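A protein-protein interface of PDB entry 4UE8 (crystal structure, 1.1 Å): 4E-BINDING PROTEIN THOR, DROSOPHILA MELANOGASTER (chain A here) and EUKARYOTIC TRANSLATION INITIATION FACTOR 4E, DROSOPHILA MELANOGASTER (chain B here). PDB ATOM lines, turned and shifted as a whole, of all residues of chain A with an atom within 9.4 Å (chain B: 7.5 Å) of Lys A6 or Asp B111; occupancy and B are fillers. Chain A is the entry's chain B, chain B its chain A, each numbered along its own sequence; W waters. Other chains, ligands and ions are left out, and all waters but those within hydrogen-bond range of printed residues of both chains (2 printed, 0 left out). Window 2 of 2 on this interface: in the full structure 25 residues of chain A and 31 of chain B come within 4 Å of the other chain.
N of Leu A7 is in hydrogen-bond range of SD of Met B9 (3.7 Å). The backbone NH (N) of Tyr A9 is in hydrogen-bond range of the backbone carbonyl oxygen (O) of Gly B107. The side-chain amino group (NZ) of Lys A6 is in hydrogen-bond range of the backbone carbonyl oxygen (O) of Phe B110 (2.7 Å). OG of Ser B113 sits at hydrogen-bond distance from NZ of Lys A6, at 2.8 Å.
OE1 of Glu B108 is in hydrogen-bond range of OG of Ser B113 (2.7 Å). OG of Ser B113 sits close to O of Phe B110, at 3.3 Å. The backbone NH (N) of Asp B111 sits at hydrogen-bond distance from the side-chain carboxylate (OE2) of Glu B145, 2.7 Å away. OD2 of Asp B111 lies within salt-bridge range of NZ of Lys B149. The backbone NH (N) of Lys A6 lies within hydrogen-bond range of the side-chain sulfur (SD) of Met A4.
Met A4 touches Met B9 (CE to CE, 3.6 Å). CE of Met B9 touches CG of Lys A6, at 3.8 Å. Glu B108 touches Lys A6. O of Asp B111 touches NZ of Lys A6, 3.7 Å away. Leu A7 touches Glu B108. CA of Ile A8 touches O of Gly B107, at 3.2 Å. CG1 of Ile A8 touches O of Glu B108, at 3.8 Å.
Of chain A, only Lys A6 comes within 4 Å of Asp B111. No residue of chain A comes within 4 Å of His B112. Of the printed residues of chain B, Tyr A9 touches Gly B107 (2.9 Å). Of the printed residues of chain A, Phe B110 touches Lys A6 (2.7 Å). Glu B141 touches none of the printed residues of chain A. Thr A5 touches none of the printed residues of chain B. The nearest printed residue of chain B that does not touch Lys A6 is His B112 (4.9 Å). The nearest printed residue of chain A that does not touch Ser B113 is Ile A8 (6.3 Å).
Of the 15 printed residues of chain B, 6 touch a printed residue of chain A. Printed residues of chain B that touch a printed residue of chain A: Met B9, Gly B107, Glu B108, Phe B110, Asp B111 and Ser B113. Hydrophobic or aromatic side chains of chain B within 4 Å of the printed part of chain A: Met B9. Printed residues of chain A that touch a printed residue of chain B: Met A4, Lys A6, Leu A7, Ile A8 and Tyr A9. Among the printed residues, 11 pairs touch across the chains.
Water W1 bridges the backbone carbonyl oxygen (O) of Leu A7 (2.9 Å) and the backbone NH (N) of Met B9 (2.9 Å). Water W2 bridges NZ of Lys A6 (3.1 Å) and OD1 of Asp B111 (3.3 Å).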
ATOM      1  N   HIS A   3      18.079  -2.611   2.577  1.00  0.00           N
ATOM      2  CA  HIS A   3      18.766  -1.463   3.156  1.00  0.00           C
ATOM      3  C   HIS A   3      19.172  -0.505   2.057  1.00  0.00           C
ATOM      4  O   HIS A   3      19.980  -0.843   1.197  1.00  0.00           O
ATOM      5  CB  HIS A   3      20.007  -1.910   3.919  1.00  0.00           C
ATOM      6  CG  HIS A   3      19.716  -2.909   4.990  1.00  0.00           C
ATOM      7  ND1 HIS A   3      20.435  -4.075   5.130  1.00  0.00           N
ATOM      8  CD2 HIS A   3      18.774  -2.923   5.960  1.00  0.00           C
ATOM      9  CE1 HIS A   3      19.953  -4.761   6.150  1.00  0.00           C
ATOM     10  NE2 HIS A   3      18.943  -4.088   6.669  1.00  0.00           N
ATOM     11  N   MET A   4      18.608   0.695   2.083  1.00  0.00           N
ATOM     12  CA  MET A   4      18.902   1.674   1.051  1.00  0.00           C
ATOM     13  C   MET A   4      20.247   2.333   1.338  1.00  0.00           C
ATOM     14  O   MET A   4      20.617   2.536   2.493  1.00  0.00           O
ATOM     15  CB  MET A   4      17.786   2.718   0.976  1.00  0.00           C
ATOM     16  CG  MET A   4      17.752   3.488  -0.336  1.00  0.00           C
ATOM     17  SD  MET A   4      18.863   4.905  -0.340  1.00  0.00           S
ATOM     18  CE  MET A   4      17.773   6.180   0.292  1.00  0.00           C
ATOM     19  N   THR A   5      20.992   2.623   0.277  1.00  0.00           N
ATOM     20  CA  THR A   5      22.228   3.389   0.380  1.00  0.00           C
ATOM     21  C   THR A   5      22.294   4.341  -0.804  1.00  0.00           C
ATOM     22  O   THR A   5      22.334   3.913  -1.949  1.00  0.00           O
ATOM     23  CB  THR A   5      23.480   2.495   0.374  1.00  0.00           C
ATOM     24  OG1 THR A   5      23.311   1.415   1.302  1.00  0.00           O
ATOM     25  CG2 THR A   5      24.703   3.311   0.761  1.00  0.00           C
ATOM     26  N   LYS A   6      22.284   5.635  -0.507  1.00  0.00           N
ATOM     27  CA  LYS A   6      22.184   6.680  -1.511  1.00  0.00           C
ATOM     28  C   LYS A   6      23.374   6.705  -2.451  1.00  0.00           C
ATOM     29  O   LYS A   6      24.518   6.567  -2.034  1.00  0.00           O
ATOM     30  CB  LYS A   6      22.114   8.047  -0.838  1.00  0.00           C
ATOM     31  CG  LYS A   6      20.855   8.335  -0.041  1.00  0.00           C
ATOM     32  CD  LYS A   6      20.910   9.720   0.592  1.00  0.00           C
ATOM     33  CE  LYS A   6      21.165  10.831  -0.436  1.00  0.00           C
ATOM     34  NZ  LYS A   6      21.089  12.195   0.155  1.00  0.00           N
ATOM     35  N   LEU A   7      23.089   6.944  -3.725  1.00  0.00           N
ATOM     36  CA  LEU A   7      24.099   7.130  -4.751  1.00  0.00           C
ATOM     37  C   LEU A   7      24.322   8.628  -4.936  1.00  0.00           C
ATOM     38  O   LEU A   7      23.433   9.348  -5.386  1.00  0.00           O
ATOM     39  CB  LEU A   7      23.608   6.443  -6.013  1.00  0.00           C
ATOM     40  CG  LEU A   7      24.440   6.535  -7.272  1.00  0.00           C
ATOM     41  CD1 LEU A   7      25.904   6.224  -7.041  1.00  0.00           C
ATOM     42  CD2 LEU A   7      23.838   5.634  -8.348  1.00  0.00           C
ATOM     43  N   ILE A   8      25.497   9.086  -4.518  1.00  0.00           N
ATOM     44  CA  ILE A   8      25.810  10.505  -4.400  1.00  0.00           C
ATOM     45  C   ILE A   8      27.042  10.822  -5.227  1.00  0.00           C
ATOM     46  O   ILE A   8      28.027  10.086  -5.201  1.00  0.00           O
ATOM     47  CB  ILE A   8      26.102  10.886  -2.922  1.00  0.00           C
ATOM     48  CG1 ILE A   8      24.881  10.612  -2.047  1.00  0.00           C
ATOM     49  CG2 ILE A   8      26.542  12.333  -2.795  1.00  0.00           C
ATOM     50  CD1 ILE A   8      25.174  10.628  -0.556  1.00  0.00           C
ATOM     51  N   TYR A   9      26.975  11.937  -5.954  1.00  0.00           N
ATOM     52  CA  TYR A   9      28.120  12.446  -6.693  1.00  0.00           C
ATOM     53  C   TYR A   9      28.411  13.873  -6.305  1.00  0.00           C
ATOM     54  O   TYR A   9      27.502  14.703  -6.169  1.00  0.00           O
ATOM     55  CB  TYR A   9      27.879  12.446  -8.193  1.00  0.00           C
ATOM     56  CG  TYR A   9      27.643  11.092  -8.816  1.00  0.00           C
ATOM     57  CD1 TYR A   9      28.672  10.168  -8.958  1.00  0.00           C
ATOM     58  CD2 TYR A   9      26.400  10.740  -9.287  1.00  0.00           C
ATOM     59  CE1 TYR A   9      28.452   8.942  -9.546  1.00  0.00           C
ATOM     60  CE2 TYR A   9      26.175   9.530  -9.892  1.00  0.00           C
ATOM     61  CZ  TYR A   9      27.208   8.630 -10.026  1.00  0.00           C
ATOM     62  OH  TYR A   9      27.006   7.417 -10.634  1.00  0.00           O
ATOM     63  N   MET B   9      20.981   8.350  -8.849  1.00  0.00           N
ATOM     64  CA  MET B   9      20.071   7.741  -7.906  1.00  0.00           C
ATOM     65  C   MET B   9      18.631   7.800  -8.402  1.00  0.00           C
ATOM     66  O   MET B   9      17.877   6.832  -8.232  1.00  0.00           O
ATOM     67  CB  MET B   9      20.179   8.417  -6.554  1.00  0.00           C
ATOM     68  CG  MET B   9      19.425   7.679  -5.487  1.00  0.00           C
ATOM     69  SD  MET B   9      19.710   8.407  -3.879  1.00  0.00           S
ATOM     70  CE  MET B   9      18.463   7.555  -2.921  1.00  0.00           C
ATOM     71  N   GLY B 107      23.114  14.916  -8.282  1.00  0.00           N
ATOM     72  CA  GLY B 107      24.134  14.270  -7.481  1.00  0.00           C
ATOM     73  C   GLY B 107      23.692  13.917  -6.072  1.00  0.00           C
ATOM     74  O   GLY B 107      24.459  13.304  -5.344  1.00  0.00           O
ATOM     75  N   GLU B 108      22.478  14.312  -5.683  1.00  0.00           N
ATOM     76  CA  GLU B 108      21.916  13.977  -4.373  1.00  0.00           C
ATOM     77  C   GLU B 108      22.778  14.602  -3.281  1.00  0.00           C
ATOM     78  O   GLU B 108      23.086  13.970  -2.284  1.00  0.00           O
ATOM     79  CB  GLU B 108      21.735  12.465  -4.200  1.00  0.00           C
ATOM     80  CG  GLU B 108      20.892  11.815  -5.302  1.00  0.00           C
ATOM     81  CD  GLU B 108      19.412  12.147  -5.259  1.00  0.00           C
ATOM     82  OE1 GLU B 108      18.898  12.535  -4.189  1.00  0.00           O
ATOM     83  OE2 GLU B 108      18.751  12.003  -6.310  1.00  0.00           O
ATOM     84  N   ALA B 109      23.106  15.880  -3.464  1.00  0.00           N
ATOM     85  CA  ALA B 109      24.035  16.569  -2.571  1.00  0.00           C
ATOM     86  C   ALA B 109      23.465  16.860  -1.186  1.00  0.00           C
ATOM     87  O   ALA B 109      24.215  17.156  -0.265  1.00  0.00           O
ATOM     88  CB  ALA B 109      24.502  17.857  -3.212  1.00  0.00           C
ATOM     89  N   PHE B 110      22.152  16.799  -1.038  1.00  0.00           N
ATOM     90  CA  PHE B 110      21.513  17.133   0.239  1.00  0.00           C
ATOM     91  C   PHE B 110      21.328  15.892   1.107  1.00  0.00           C
ATOM     92  O   PHE B 110      20.999  14.824   0.598  1.00  0.00           O
ATOM     93  CB  PHE B 110      20.155  17.804  -0.008  1.00  0.00           C
ATOM     94  CG  PHE B 110      20.199  18.932  -1.006  1.00  0.00           C
ATOM     95  CD1 PHE B 110      20.622  20.189  -0.621  1.00  0.00           C
ATOM     96  CD2 PHE B 110      19.821  18.735  -2.328  1.00  0.00           C
ATOM     97  CE1 PHE B 110      20.674  21.228  -1.530  1.00  0.00           C
ATOM     98  CE2 PHE B 110      19.875  19.776  -3.242  1.00  0.00           C
ATOM     99  CZ  PHE B 110      20.301  21.021  -2.837  1.00  0.00           C
ATOM    100  N   ASP B 111      21.540  16.027   2.413  1.00  0.00           N
ATOM    101  CA  ASP B 111      21.262  14.925   3.328  1.00  0.00           C
ATOM    102  C   ASP B 111      19.797  14.521   3.195  1.00  0.00           C
ATOM    103  O   ASP B 111      19.457  13.337   3.260  1.00  0.00           O
ATOM    104  CB  ASP B 111      21.563  15.308   4.784  1.00  0.00           C
ATOM    105  CG  ASP B 111      23.048  15.449   5.061  1.00  0.00           C
ATOM    106  OD1 ASP B 111      23.859  14.831   4.335  1.00  0.00           O
ATOM    107  OD2 ASP B 111      23.403  16.173   6.015  1.00  0.00           O
ATOM    108  N   HIS B 112      18.934  15.516   3.023  1.00  0.00           N
ATOM    109  CA  HIS B 112      17.510  15.274   2.849  1.00  0.00           C
ATOM    110  C   HIS B 112      17.133  15.410   1.386  1.00  0.00           C
ATOM    111  O   HIS B 112      16.049  15.890   1.069  1.00  0.00           O
ATOM    112  CB  HIS B 112      16.681  16.258   3.670  1.00  0.00           C
ATOM    113  CG  HIS B 112      16.917  16.154   5.137  1.00  0.00           C
ATOM    114  ND1 HIS B 112      17.974  16.774   5.767  1.00  0.00           N
ATOM    115  CD2 HIS B 112      16.245  15.482   6.096  1.00  0.00           C
ATOM    116  CE1 HIS B 112      17.938  16.492   7.055  1.00  0.00           C
ATOM    117  NE2 HIS B 112      16.897  15.711   7.281  1.00  0.00           N
ATOM    118  N   SER B 113      18.028  14.990   0.492  1.00  0.00           N
ATOM    119  CA  SER B 113      17.742  15.046  -0.938  1.00  0.00           C
ATOM    120  C   SER B 113      16.438  14.323  -1.282  1.00  0.00           C
ATOM    121  O   SER B 113      15.822  14.617  -2.287  1.00  0.00           O
ATOM    122  CB  SER B 113      18.900  14.479  -1.759  1.00  0.00           C
ATOM    123  OG  SER B 113      19.079  13.096  -1.511  1.00  0.00           O
ATOM    124  N   ASP B 114      16.024  13.369  -0.456  1.00  0.00           N
ATOM    125  CA  ASP B 114      14.722  12.714  -0.638  1.00  0.00           C
ATOM    126  C   ASP B 114      13.524  13.691  -0.653  1.00  0.00           C
ATOM    127  O   ASP B 114      12.530  13.447  -1.342  1.00  0.00           O
ATOM    128  CB  ASP B 114      14.517  11.630   0.420  1.00  0.00           C
ATOM    129  CG  ASP B 114      14.621  12.169   1.827  1.00  0.00           C
ATOM    130  OD1 ASP B 114      15.757  12.438   2.277  1.00  0.00           O
ATOM    131  OD2 ASP B 114      13.569  12.323   2.484  1.00  0.00           O
ATOM    132  N   GLN B 115      13.628  14.792   0.089  1.00  0.00           N
ATOM    133  CA  GLN B 115      12.579  15.828   0.158  1.00  0.00           C
ATOM    134  C   GLN B 115      12.564  16.760  -1.042  1.00  0.00           C
ATOM    135  O   GLN B 115      11.681  17.609  -1.175  1.00  0.00           O
ATOM    136  CB  GLN B 115      12.754  16.653   1.433  1.00  0.00           C
ATOM    137  CG  GLN B 115      12.089  16.049   2.653  1.00  0.00           C
ATOM    138  CD  GLN B 115      10.591  16.230   2.614  1.00  0.00           C
ATOM    139  OE1 GLN B 115      10.094  17.346   2.426  1.00  0.00           O
ATOM    140  NE2 GLN B 115       9.860  15.139   2.752  1.00  0.00           N
ATOM    141  N   GLU B 141      13.631  20.093   9.641  1.00  0.00           N
ATOM    142  CA  GLU B 141      15.008  19.669   9.520  1.00  0.00           C
ATOM    143  C   GLU B 141      15.434  19.644   8.056  1.00  0.00           C
ATOM    144  O   GLU B 141      16.524  20.104   7.708  1.00  0.00           O
ATOM    145  CB  GLU B 141      15.159  18.294  10.151  1.00  0.00           C
ATOM    146  CG  GLU B 141      16.547  17.723  10.112  1.00  0.00           C
ATOM    147  CD  GLU B 141      16.578  16.299  10.630  1.00  0.00           C
ATOM    148  OE1 GLU B 141      16.549  16.113  11.859  1.00  0.00           O
ATOM    149  OE2 GLU B 141      16.610  15.358   9.810  1.00  0.00           O
ATOM    150  N   ALA B 142      14.570  19.103   7.202  1.00  0.00           N
ATOM    151  CA  ALA B 142      14.880  19.009   5.779  1.00  0.00           C
ATOM    152  C   ALA B 142      14.952  20.383   5.126  1.00  0.00           C
ATOM    153  O   ALA B 142      15.884  20.669   4.367  1.00  0.00           O
ATOM    154  CB  ALA B 142      13.858  18.154   5.075  1.00  0.00           C
ATOM    155  N   GLU B 145      18.192  22.176   6.203  1.00  0.00           N
ATOM    156  CA  GLU B 145      19.407  21.584   5.672  1.00  0.00           C
ATOM    157  C   GLU B 145      19.561  21.925   4.194  1.00  0.00           C
ATOM    158  O   GLU B 145      20.645  22.298   3.736  1.00  0.00           O
ATOM    159  CB  GLU B 145      19.408  20.077   5.882  1.00  0.00           C
ATOM    160  CG  GLU B 145      20.722  19.432   5.485  1.00  0.00           C
ATOM    161  CD  GLU B 145      20.670  18.656   4.184  1.00  0.00           C
ATOM    162  OE1 GLU B 145      19.583  18.196   3.765  1.00  0.00           O
ATOM    163  OE2 GLU B 145      21.752  18.491   3.584  1.00  0.00           O
ATOM    164  N   ILE B 146      18.471  21.800   3.451  1.00  0.00           N
ATOM    165  CA  ILE B 146      18.503  22.103   2.024  1.00  0.00           C
ATOM    166  C   ILE B 146      18.853  23.572   1.783  1.00  0.00           C
ATOM    167  O   ILE B 146      19.704  23.878   0.958  1.00  0.00           O
ATOM    168  CB  ILE B 146      17.176  21.709   1.361  1.00  0.00           C
ATOM    169  CG1 ILE B 146      17.075  20.184   1.336  1.00  0.00           C
ATOM    170  CG2 ILE B 146      17.073  22.245  -0.065  1.00  0.00           C
ATOM    171  CD1 ILE B 146      15.685  19.650   1.104  1.00  0.00           C
ATOM    172  N   LYS B 149      22.615  24.254   2.614  1.00  0.00           N
ATOM    173  CA  LYS B 149      23.511  23.706   1.614  1.00  0.00           C
ATOM    174  C   LYS B 149      23.442  24.484   0.302  1.00  0.00           C
ATOM    175  O   LYS B 149      24.458  24.643  -0.374  1.00  0.00           O
ATOM    176  CB  LYS B 149      23.226  22.229   1.390  1.00  0.00           C
ATOM    177  CG  LYS B 149      23.787  21.354   2.497  1.00  0.00           C
ATOM    178  CD  LYS B 149      24.305  20.025   1.978  1.00  0.00           C
ATOM    179  CE  LYS B 149      25.027  19.256   3.070  1.00  0.00           C
ATOM    180  NZ  LYS B 149      24.194  19.116   4.299  1.00  0.00           N
HETATM  181  O   HOH W   1      22.890  10.323  -8.013  1.00  0.00           O
HETATM  182  O   HOH W   2      23.534  12.440   2.115  1.00  0.00           O
